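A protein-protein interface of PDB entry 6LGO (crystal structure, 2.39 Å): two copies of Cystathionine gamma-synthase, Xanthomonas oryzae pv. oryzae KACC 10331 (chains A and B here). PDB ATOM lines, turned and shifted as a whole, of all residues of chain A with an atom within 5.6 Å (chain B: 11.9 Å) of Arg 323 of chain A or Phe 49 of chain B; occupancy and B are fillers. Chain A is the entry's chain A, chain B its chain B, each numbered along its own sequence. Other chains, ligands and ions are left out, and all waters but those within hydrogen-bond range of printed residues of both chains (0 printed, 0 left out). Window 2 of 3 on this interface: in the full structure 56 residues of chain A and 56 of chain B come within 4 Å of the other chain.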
ATOM      1  N   GLY A 318     -23.090  15.479  37.905  1.00  0.00           N
ATOM      2  CA  GLY A 318     -24.366  15.190  37.223  1.00  0.00           C
ATOM      3  C   GLY A 318     -24.585  16.085  36.014  1.00  0.00           C
ATOM      4  O   GLY A 318     -23.596  16.517  35.360  1.00  0.00           O
ATOM      5  N   GLU A 319     -25.852  16.292  35.670  1.00  0.00           N
ATOM      6  CA  GLU A 319     -26.271  16.874  34.384  1.00  0.00           C
ATOM      7  C   GLU A 319     -25.809  18.339  34.304  1.00  0.00           C
ATOM      8  O   GLU A 319     -25.450  18.814  33.186  1.00  0.00           O
ATOM      9  CB  GLU A 319     -27.785  16.718  34.177  1.00  0.00           C
ATOM     10  CG  GLU A 319     -28.187  16.930  32.705  1.00  0.00           C
ATOM     11  CD  GLU A 319     -29.669  16.954  32.332  1.00  0.00           C
ATOM     12  OE1 GLU A 319     -30.003  16.430  31.250  1.00  0.00           O
ATOM     13  OE2 GLU A 319     -30.486  17.503  33.095  1.00  0.00           O
ATOM     14  N   ALA A 320     -25.803  19.069  35.421  1.00  0.00           N
ATOM     15  CA  ALA A 320     -25.419  20.510  35.438  1.00  0.00           C
ATOM     16  C   ALA A 320     -23.938  20.606  35.005  1.00  0.00           C
ATOM     17  O   ALA A 320     -23.576  21.588  34.340  1.00  0.00           O
ATOM     18  CB  ALA A 320     -25.636  21.163  36.813  1.00  0.00           C
ATOM     19  N   ALA A 321     -23.103  19.656  35.426  1.00  0.00           N
ATOM     20  CA  ALA A 321     -21.665  19.719  35.108  1.00  0.00           C
ATOM     21  C   ALA A 321     -21.442  19.471  33.599  1.00  0.00           C
ATOM     22  O   ALA A 321     -20.646  20.224  33.003  1.00  0.00           O
ATOM     23  CB  ALA A 321     -20.914  18.759  35.974  1.00  0.00           C
ATOM     24  N   VAL A 322     -22.161  18.496  33.026  1.00  0.00           N
ATOM     25  CA  VAL A 322     -22.180  18.157  31.578  1.00  0.00           C
ATOM     26  C   VAL A 322     -22.558  19.396  30.758  1.00  0.00           C
ATOM     27  O   VAL A 322     -21.762  19.805  29.925  1.00  0.00           O
ATOM     28  CB  VAL A 322     -23.143  16.980  31.336  1.00  0.00           C
ATOM     29  CG1 VAL A 322     -23.385  16.731  29.857  1.00  0.00           C
ATOM     30  CG2 VAL A 322     -22.660  15.689  32.002  1.00  0.00           C
ATOM     31  N   ARG A 323     -23.692  20.024  31.069  1.00  0.00           N
ATOM     32  CA  ARG A 323     -24.251  21.220  30.384  1.00  0.00           C
ATOM     33  C   ARG A 323     -23.189  22.314  30.475  1.00  0.00           C
ATOM     34  O   ARG A 323     -22.866  22.926  29.452  1.00  0.00           O
ATOM     35  CB  ARG A 323     -25.676  21.543  30.879  1.00  0.00           C
ATOM     36  CG  ARG A 323     -26.296  22.852  30.344  1.00  0.00           C
ATOM     37  CD  ARG A 323     -27.778  22.762  29.923  1.00  0.00           C
ATOM     38  NE  ARG A 323     -28.329  21.598  30.668  1.00  0.00           N
ATOM     39  CZ  ARG A 323     -29.287  20.750  30.238  1.00  0.00           C
ATOM     40  NH1 ARG A 323     -29.845  20.875  29.050  1.00  0.00           N
ATOM     41  NH2 ARG A 323     -29.651  19.728  30.994  1.00  0.00           N
ATOM     42  N   ALA A 324     -22.527  22.501  31.603  1.00  0.00           N
ATOM     43  CA  ALA A 324     -21.570  23.624  31.703  1.00  0.00           C
ATOM     44  C   ALA A 324     -20.265  23.276  30.940  1.00  0.00           C
ATOM     45  O   ALA A 324     -19.644  24.204  30.333  1.00  0.00           O
ATOM     46  CB  ALA A 324     -21.337  23.968  33.157  1.00  0.00           C
ATOM     47  N   PHE A 325     -19.836  22.000  30.963  1.00  0.00           N
ATOM     48  CA  PHE A 325     -18.635  21.561  30.224  1.00  0.00           C
ATOM     49  C   PHE A 325     -18.883  21.793  28.725  1.00  0.00           C
ATOM     50  O   PHE A 325     -18.031  22.380  28.037  1.00  0.00           O
ATOM     51  CB  PHE A 325     -18.309  20.104  30.544  1.00  0.00           C
ATOM     52  CG  PHE A 325     -17.124  19.569  29.799  1.00  0.00           C
ATOM     53  CD1 PHE A 325     -17.269  19.061  28.511  1.00  0.00           C
ATOM     54  CD2 PHE A 325     -15.879  19.561  30.391  1.00  0.00           C
ATOM     55  CE1 PHE A 325     -16.163  18.578  27.821  1.00  0.00           C
ATOM     56  CE2 PHE A 325     -14.782  19.089  29.693  1.00  0.00           C
ATOM     57  CZ  PHE A 325     -14.916  18.616  28.405  1.00  0.00           C
ATOM     58  N   VAL A 326     -20.043  21.423  28.226  1.00  0.00           N
ATOM     59  CA  VAL A 326     -20.276  21.390  26.751  1.00  0.00           C
ATOM     60  C   VAL A 326     -20.475  22.806  26.175  1.00  0.00           C
ATOM     61  O   VAL A 326     -19.881  23.123  25.105  1.00  0.00           O
ATOM     62  CB  VAL A 326     -21.451  20.444  26.421  1.00  0.00           C
ATOM     63  CG1 VAL A 326     -21.930  20.606  25.010  1.00  0.00           C
ATOM     64  CG2 VAL A 326     -21.035  19.012  26.650  1.00  0.00           C
ATOM     65  N   ASP A 327     -21.212  23.649  26.884  1.00  0.00           N
ATOM     66  CA  ASP A 327     -21.612  25.005  26.412  1.00  0.00           C
ATOM     67  C   ASP A 327     -20.418  25.925  26.686  1.00  0.00           C
ATOM     68  O   ASP A 327     -20.055  26.062  27.811  1.00  0.00           O
ATOM     69  CB  ASP A 327     -23.015  25.380  26.943  1.00  0.00           C
ATOM     70  CG  ASP A 327     -24.170  24.447  26.418  1.00  0.00           C
ATOM     71  OD1 ASP A 327     -24.190  24.065  25.189  1.00  0.00           O
ATOM     72  OD2 ASP A 327     -25.059  24.019  27.257  1.00  0.00           O
ATOM     73  N   LEU A 334     -20.137  20.126  19.084  1.00  0.00           N
ATOM     74  CA  LEU A 334     -21.179  19.209  19.554  1.00  0.00           C
ATOM     75  C   LEU A 334     -21.913  18.747  18.321  1.00  0.00           C
ATOM     76  O   LEU A 334     -22.645  19.578  17.694  1.00  0.00           O
ATOM     77  CB  LEU A 334     -22.082  19.964  20.517  1.00  0.00           C
ATOM     78  CG  LEU A 334     -23.206  19.071  21.048  1.00  0.00           C
ATOM     79  CD1 LEU A 334     -22.671  17.839  21.793  1.00  0.00           C
ATOM     80  CD2 LEU A 334     -24.170  19.909  21.907  1.00  0.00           C
ATOM     81  N   HIS A 347     -22.860  13.296  23.174  1.00  0.00           N
ATOM     82  CA  HIS A 347     -23.538  12.759  24.390  1.00  0.00           C
ATOM     83  C   HIS A 347     -24.328  11.530  23.948  1.00  0.00           C
ATOM     84  O   HIS A 347     -25.363  11.680  23.287  1.00  0.00           O
ATOM     85  CB  HIS A 347     -24.382  13.850  25.048  1.00  0.00           C
ATOM     86  CG  HIS A 347     -25.205  13.351  26.189  1.00  0.00           C
ATOM     87  ND1 HIS A 347     -26.590  13.207  26.076  1.00  0.00           N
ATOM     88  CD2 HIS A 347     -24.865  13.014  27.460  1.00  0.00           C
ATOM     89  CE1 HIS A 347     -27.080  12.800  27.248  1.00  0.00           C
ATOM     90  NE2 HIS A 347     -26.034  12.654  28.107  1.00  0.00           N
ATOM     91  N   SER A 350     -28.451  10.808  24.250  1.00  0.00           N
ATOM     92  CA  SER A 350     -29.358  11.710  23.482  1.00  0.00           C
ATOM     93  C   SER A 350     -28.923  11.822  21.998  1.00  0.00           C
ATOM     94  O   SER A 350     -29.642  12.432  21.216  1.00  0.00           O
ATOM     95  CB  SER A 350     -29.388  13.081  24.147  1.00  0.00           C
ATOM     96  OG  SER A 350     -28.158  13.776  23.984  1.00  0.00           O
ATOM     97  N   LEU A 371     -19.849  11.452  28.064  1.00  0.00           N
ATOM     98  CA  LEU A 371     -19.383  12.235  26.887  1.00  0.00           C
ATOM     99  C   LEU A 371     -18.325  11.445  26.112  1.00  0.00           C
ATOM    100  O   LEU A 371     -17.489  10.772  26.749  1.00  0.00           O
ATOM    101  CB  LEU A 371     -18.898  13.604  27.374  1.00  0.00           C
ATOM    102  CG  LEU A 371     -20.028  14.443  27.990  1.00  0.00           C
ATOM    103  CD1 LEU A 371     -19.428  15.642  28.695  1.00  0.00           C
ATOM    104  CD2 LEU A 371     -21.106  14.832  26.935  1.00  0.00           C
ATOM    105  N   PHE B  44     -23.906  17.863  11.350  1.00  0.00           N
ATOM    106  CA  PHE B  44     -24.503  19.201  11.608  1.00  0.00           C
ATOM    107  C   PHE B  44     -24.352  19.460  13.126  1.00  0.00           C
ATOM    108  O   PHE B  44     -24.681  18.540  13.918  1.00  0.00           O
ATOM    109  CB  PHE B  44     -25.987  19.197  11.162  1.00  0.00           C
ATOM    110  CG  PHE B  44     -26.215  18.875   9.720  1.00  0.00           C
ATOM    111  CD1 PHE B  44     -26.125  17.578   9.275  1.00  0.00           C
ATOM    112  CD2 PHE B  44     -26.326  19.882   8.793  1.00  0.00           C
ATOM    113  CE1 PHE B  44     -26.217  17.296   7.932  1.00  0.00           C
ATOM    114  CE2 PHE B  44     -26.497  19.602   7.458  1.00  0.00           C
ATOM    115  CZ  PHE B  44     -26.397  18.316   7.017  1.00  0.00           C
ATOM    116  N   SER B  45     -23.863  20.627  13.538  1.00  0.00           N
ATOM    117  CA  SER B  45     -23.811  21.050  14.948  1.00  0.00           C
ATOM    118  C   SER B  45     -25.204  20.982  15.587  1.00  0.00           C
ATOM    119  O   SER B  45     -26.247  21.097  14.891  1.00  0.00           O
ATOM    120  CB  SER B  45     -23.210  22.396  15.129  1.00  0.00           C
ATOM    121  OG  SER B  45     -23.947  23.350  14.379  1.00  0.00           O
ATOM    122  N   PHE B  46     -25.206  20.595  16.868  1.00  0.00           N
ATOM    123  CA  PHE B  46     -26.289  20.923  17.813  1.00  0.00           C
ATOM    124  C   PHE B  46     -26.144  22.402  18.213  1.00  0.00           C
ATOM    125  O   PHE B  46     -25.071  23.025  18.082  1.00  0.00           O
ATOM    126  CB  PHE B  46     -26.258  19.966  18.998  1.00  0.00           C
ATOM    127  CG  PHE B  46     -26.898  18.616  18.804  1.00  0.00           C
ATOM    128  CD1 PHE B  46     -26.614  17.833  17.687  1.00  0.00           C
ATOM    129  CD2 PHE B  46     -27.757  18.104  19.769  1.00  0.00           C
ATOM    130  CE1 PHE B  46     -27.191  16.589  17.539  1.00  0.00           C
ATOM    131  CE2 PHE B  46     -28.351  16.855  19.598  1.00  0.00           C
ATOM    132  CZ  PHE B  46     -28.041  16.091  18.504  1.00  0.00           C
ATOM    133  N   ASP B  47     -27.287  22.983  18.551  1.00  0.00           N
ATOM    134  CA  ASP B  47     -27.478  24.399  18.963  1.00  0.00           C
ATOM    135  C   ASP B  47     -27.440  24.435  20.490  1.00  0.00           C
ATOM    136  O   ASP B  47     -28.508  24.619  21.094  1.00  0.00           O
ATOM    137  CB  ASP B  47     -28.805  24.911  18.365  1.00  0.00           C
ATOM    138  CG  ASP B  47     -29.130  26.368  18.651  1.00  0.00           C
ATOM    139  OD1 ASP B  47     -28.175  27.172  18.764  1.00  0.00           O
ATOM    140  OD2 ASP B  47     -30.340  26.671  18.731  1.00  0.00           O
ATOM    141  N   GLY B  48     -26.281  24.111  21.058  1.00  0.00           N
ATOM    142  CA  GLY B  48     -26.122  23.771  22.486  1.00  0.00           C
ATOM    143  C   GLY B  48     -26.670  22.390  22.853  1.00  0.00           C
ATOM    144  O   GLY B  48     -27.460  21.791  22.098  1.00  0.00           O
ATOM    145  N   PHE B  49     -26.270  21.915  24.036  1.00  0.00           N
ATOM    146  CA  PHE B  49     -26.566  20.590  24.617  1.00  0.00           C
ATOM    147  C   PHE B  49     -28.088  20.363  24.579  1.00  0.00           C
ATOM    148  O   PHE B  49     -28.820  21.218  25.116  1.00  0.00           O
ATOM    149  CB  PHE B  49     -25.935  20.537  26.025  1.00  0.00           C
ATOM    150  CG  PHE B  49     -26.090  19.209  26.712  1.00  0.00           C
ATOM    151  CD1 PHE B  49     -25.286  18.142  26.350  1.00  0.00           C
ATOM    152  CD2 PHE B  49     -27.151  18.978  27.582  1.00  0.00           C
ATOM    153  CE1 PHE B  49     -25.521  16.886  26.897  1.00  0.00           C
ATOM    154  CE2 PHE B  49     -27.396  17.717  28.114  1.00  0.00           C
ATOM    155  CZ  PHE B  49     -26.543  16.681  27.799  1.00  0.00           C
ATOM    156  N   GLY B  50     -28.514  19.205  24.048  1.00  0.00           N
ATOM    157  CA  GLY B  50     -29.899  18.693  23.970  1.00  0.00           C
ATOM    158  C   GLY B  50     -30.742  19.285  22.833  1.00  0.00           C
ATOM    159  O   GLY B  50     -31.908  18.940  22.777  1.00  0.00           O
ATOM    160  N   ASN B  51     -30.194  20.188  21.997  1.00  0.00           N
ATOM    161  CA  ASN B  51     -30.951  20.950  20.957  1.00  0.00           C
ATOM    162  C   ASN B  51     -30.511  20.544  19.559  1.00  0.00           C
ATOM    163  O   ASN B  51     -29.668  21.225  18.944  1.00  0.00           O
ATOM    164  CB  ASN B  51     -30.779  22.475  21.113  1.00  0.00           C
ATOM    165  CG  ASN B  51     -31.289  22.953  22.466  1.00  0.00           C
ATOM    166  OD1 ASN B  51     -30.627  23.780  23.100  1.00  0.00           O
ATOM    167  ND2 ASN B  51     -32.396  22.351  22.932  1.00  0.00           N
ATOM    168  N   LYS B  52     -31.000  19.404  19.120  1.00  0.00           N
ATOM    169  CA  LYS B  52     -30.859  18.948  17.737  1.00  0.00           C
ATOM    170  C   LYS B  52     -31.401  20.084  16.837  1.00  0.00           C
ATOM    171  O   LYS B  52     -32.483  20.576  17.098  1.00  0.00           O
ATOM    172  CB  LYS B  52     -31.644  17.644  17.575  1.00  0.00           C
ATOM    173  CG  LYS B  52     -31.231  16.878  16.324  1.00  0.00           C
ATOM    174  CD  LYS B  52     -31.906  15.545  16.119  1.00  0.00           C
ATOM    175  CE  LYS B  52     -33.405  15.632  15.919  1.00  0.00           C
ATOM    176  NZ  LYS B  52     -33.692  16.496  14.762  1.00  0.00           N
ATOM    177  N   ARG B  53     -30.671  20.494  15.814  1.00  0.00           N
ATOM    178  CA  ARG B  53     -31.244  21.337  14.721  1.00  0.00           C
ATOM    179  C   ARG B  53     -32.206  20.481  13.884  1.00  0.00           C
ATOM    180  O   ARG B  53     -32.286  19.262  14.159  1.00  0.00           O
ATOM    181  CB  ARG B  53     -30.122  21.894  13.836  1.00  0.00           C
ATOM    182  CG  ARG B  53     -29.209  22.849  14.582  1.00  0.00           C
ATOM    183  CD  ARG B  53     -28.158  23.418  13.689  1.00  0.00           C
ATOM    184  NE  ARG B  53     -27.032  23.962  14.444  1.00  0.00           N
ATOM    185  CZ  ARG B  53     -26.968  25.184  15.014  1.00  0.00           C
ATOM    186  NH1 ARG B  53     -28.016  25.960  15.029  1.00  0.00           N
ATOM    187  NH2 ARG B  53     -25.889  25.580  15.665  1.00  0.00           N
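The side-chain carboxylate (OD1) of Asp 327 of chain A is in hydrogen-bond range of the backbone NH (N) of Phe 49 of chain B, 3.2 Å away.
The backbone NH of Phe 46 of chain B is in hydrogen-bond range of the backbone carbonyl oxygen of Leu 334 of chain A, at 2.9 Å.
The guanidinium group (NH2) of Arg 323 of chain A is in salt-bridge range of the side-chain carboxylate (OE2) of Glu 319 of chain A (3.2 Å).
The side-chain hydroxyl of Ser 350 of chain A sits at hydrogen-bond distance from a ring nitrogen (ND1) of His 347 of chain A.
O of Ser 45 of chain B is in hydrogen-bond range of NE of Arg 53 of chain B (3.0 Å).
Among the printed residues, merely in contact across the chains: Leu 334 of chain A with Ser 45 of chain B, Asp 327 of chain A with Gly 48 of chain B, Leu 334 of chain A with Phe 49 of chain B, Arg 323 of chain A with Phe 49 of chain B, His 347 of chain A with Phe 49 of chain B, Leu 334 of chain A with Gly 48 of chain B and Val 322 of chain A with Phe 49 of chain B.
Phe 49 of chain B touches just these residues of chain A: Val 322, Arg 323, Asp 327, Leu 334 and His 347.
No residue of chain B comes within 4 Å of Glu 319 of chain A.
Ala 320 of chain A touches none of the printed residues of chain B.
Ala 321 of chain A touches none of the printed residues of chain B.
Of chain B, only Phe 49 (3.7 Å) comes within 4 Å of Val 322 of chain A.
No residue of chain B comes within 4 Å of Val 326 of chain A.
Of chain B, only Gly 48 (3.3 Å) and Phe 49 (3.2 Å) come within 4 Å of Asp 327 of chain A.
His 347 of chain A touches just one residue of chain B: Phe 49 (3.6 Å).
Printed residues of chain A within 4 Å of Ser 45 of chain B: Leu 334 (3.3 Å).
Of the printed residues of chain A, Gly 48 of chain B touches Asp 327 and Leu 334.
Of the printed residues of chain B, Leu 334 of chain A touches Ser 45 (3.3 Å), Phe 46 (2.9 Å), Gly 48 (3.6 Å) and Phe 49 (3.6 Å).
Of the printed residues of chain A, Phe 46 of chain B touches Leu 334 (2.9 Å).
Gly 318 of chain A touches none of the printed residues of chain B.
Phe 44 of chain B touches none of the printed residues of chain A.
The nearest residue of chain B that does not touch Arg 323 of chain A is Gly 50 of chain B (5.4 Å).
The nearest residue of chain A that does not touch Phe 49 of chain B is Val 326 of chain A (4.1 Å).
The nearest printed residue of chain A that does not touch Phe 46 of chain B is Ser 350 of chain A (4.8 Å).
Hydrophobic or aromatic side chains of chain B within 4 Å of the printed part of chain A: Phe 46 and Phe 49.
Printed residues of chain A that touch a printed residue of chain B: Val 322, Arg 323, Asp 327, Leu 334 and His 347.
Hydrophobic or aromatic side chains of chain A that line the printed part of chain B: Val 322, Leu 334 and His 347.
No position is printed for both chains.
Of the 9 pairs that touch across the chains among the printed residues, none has its exchanged pair printed and touching as well.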
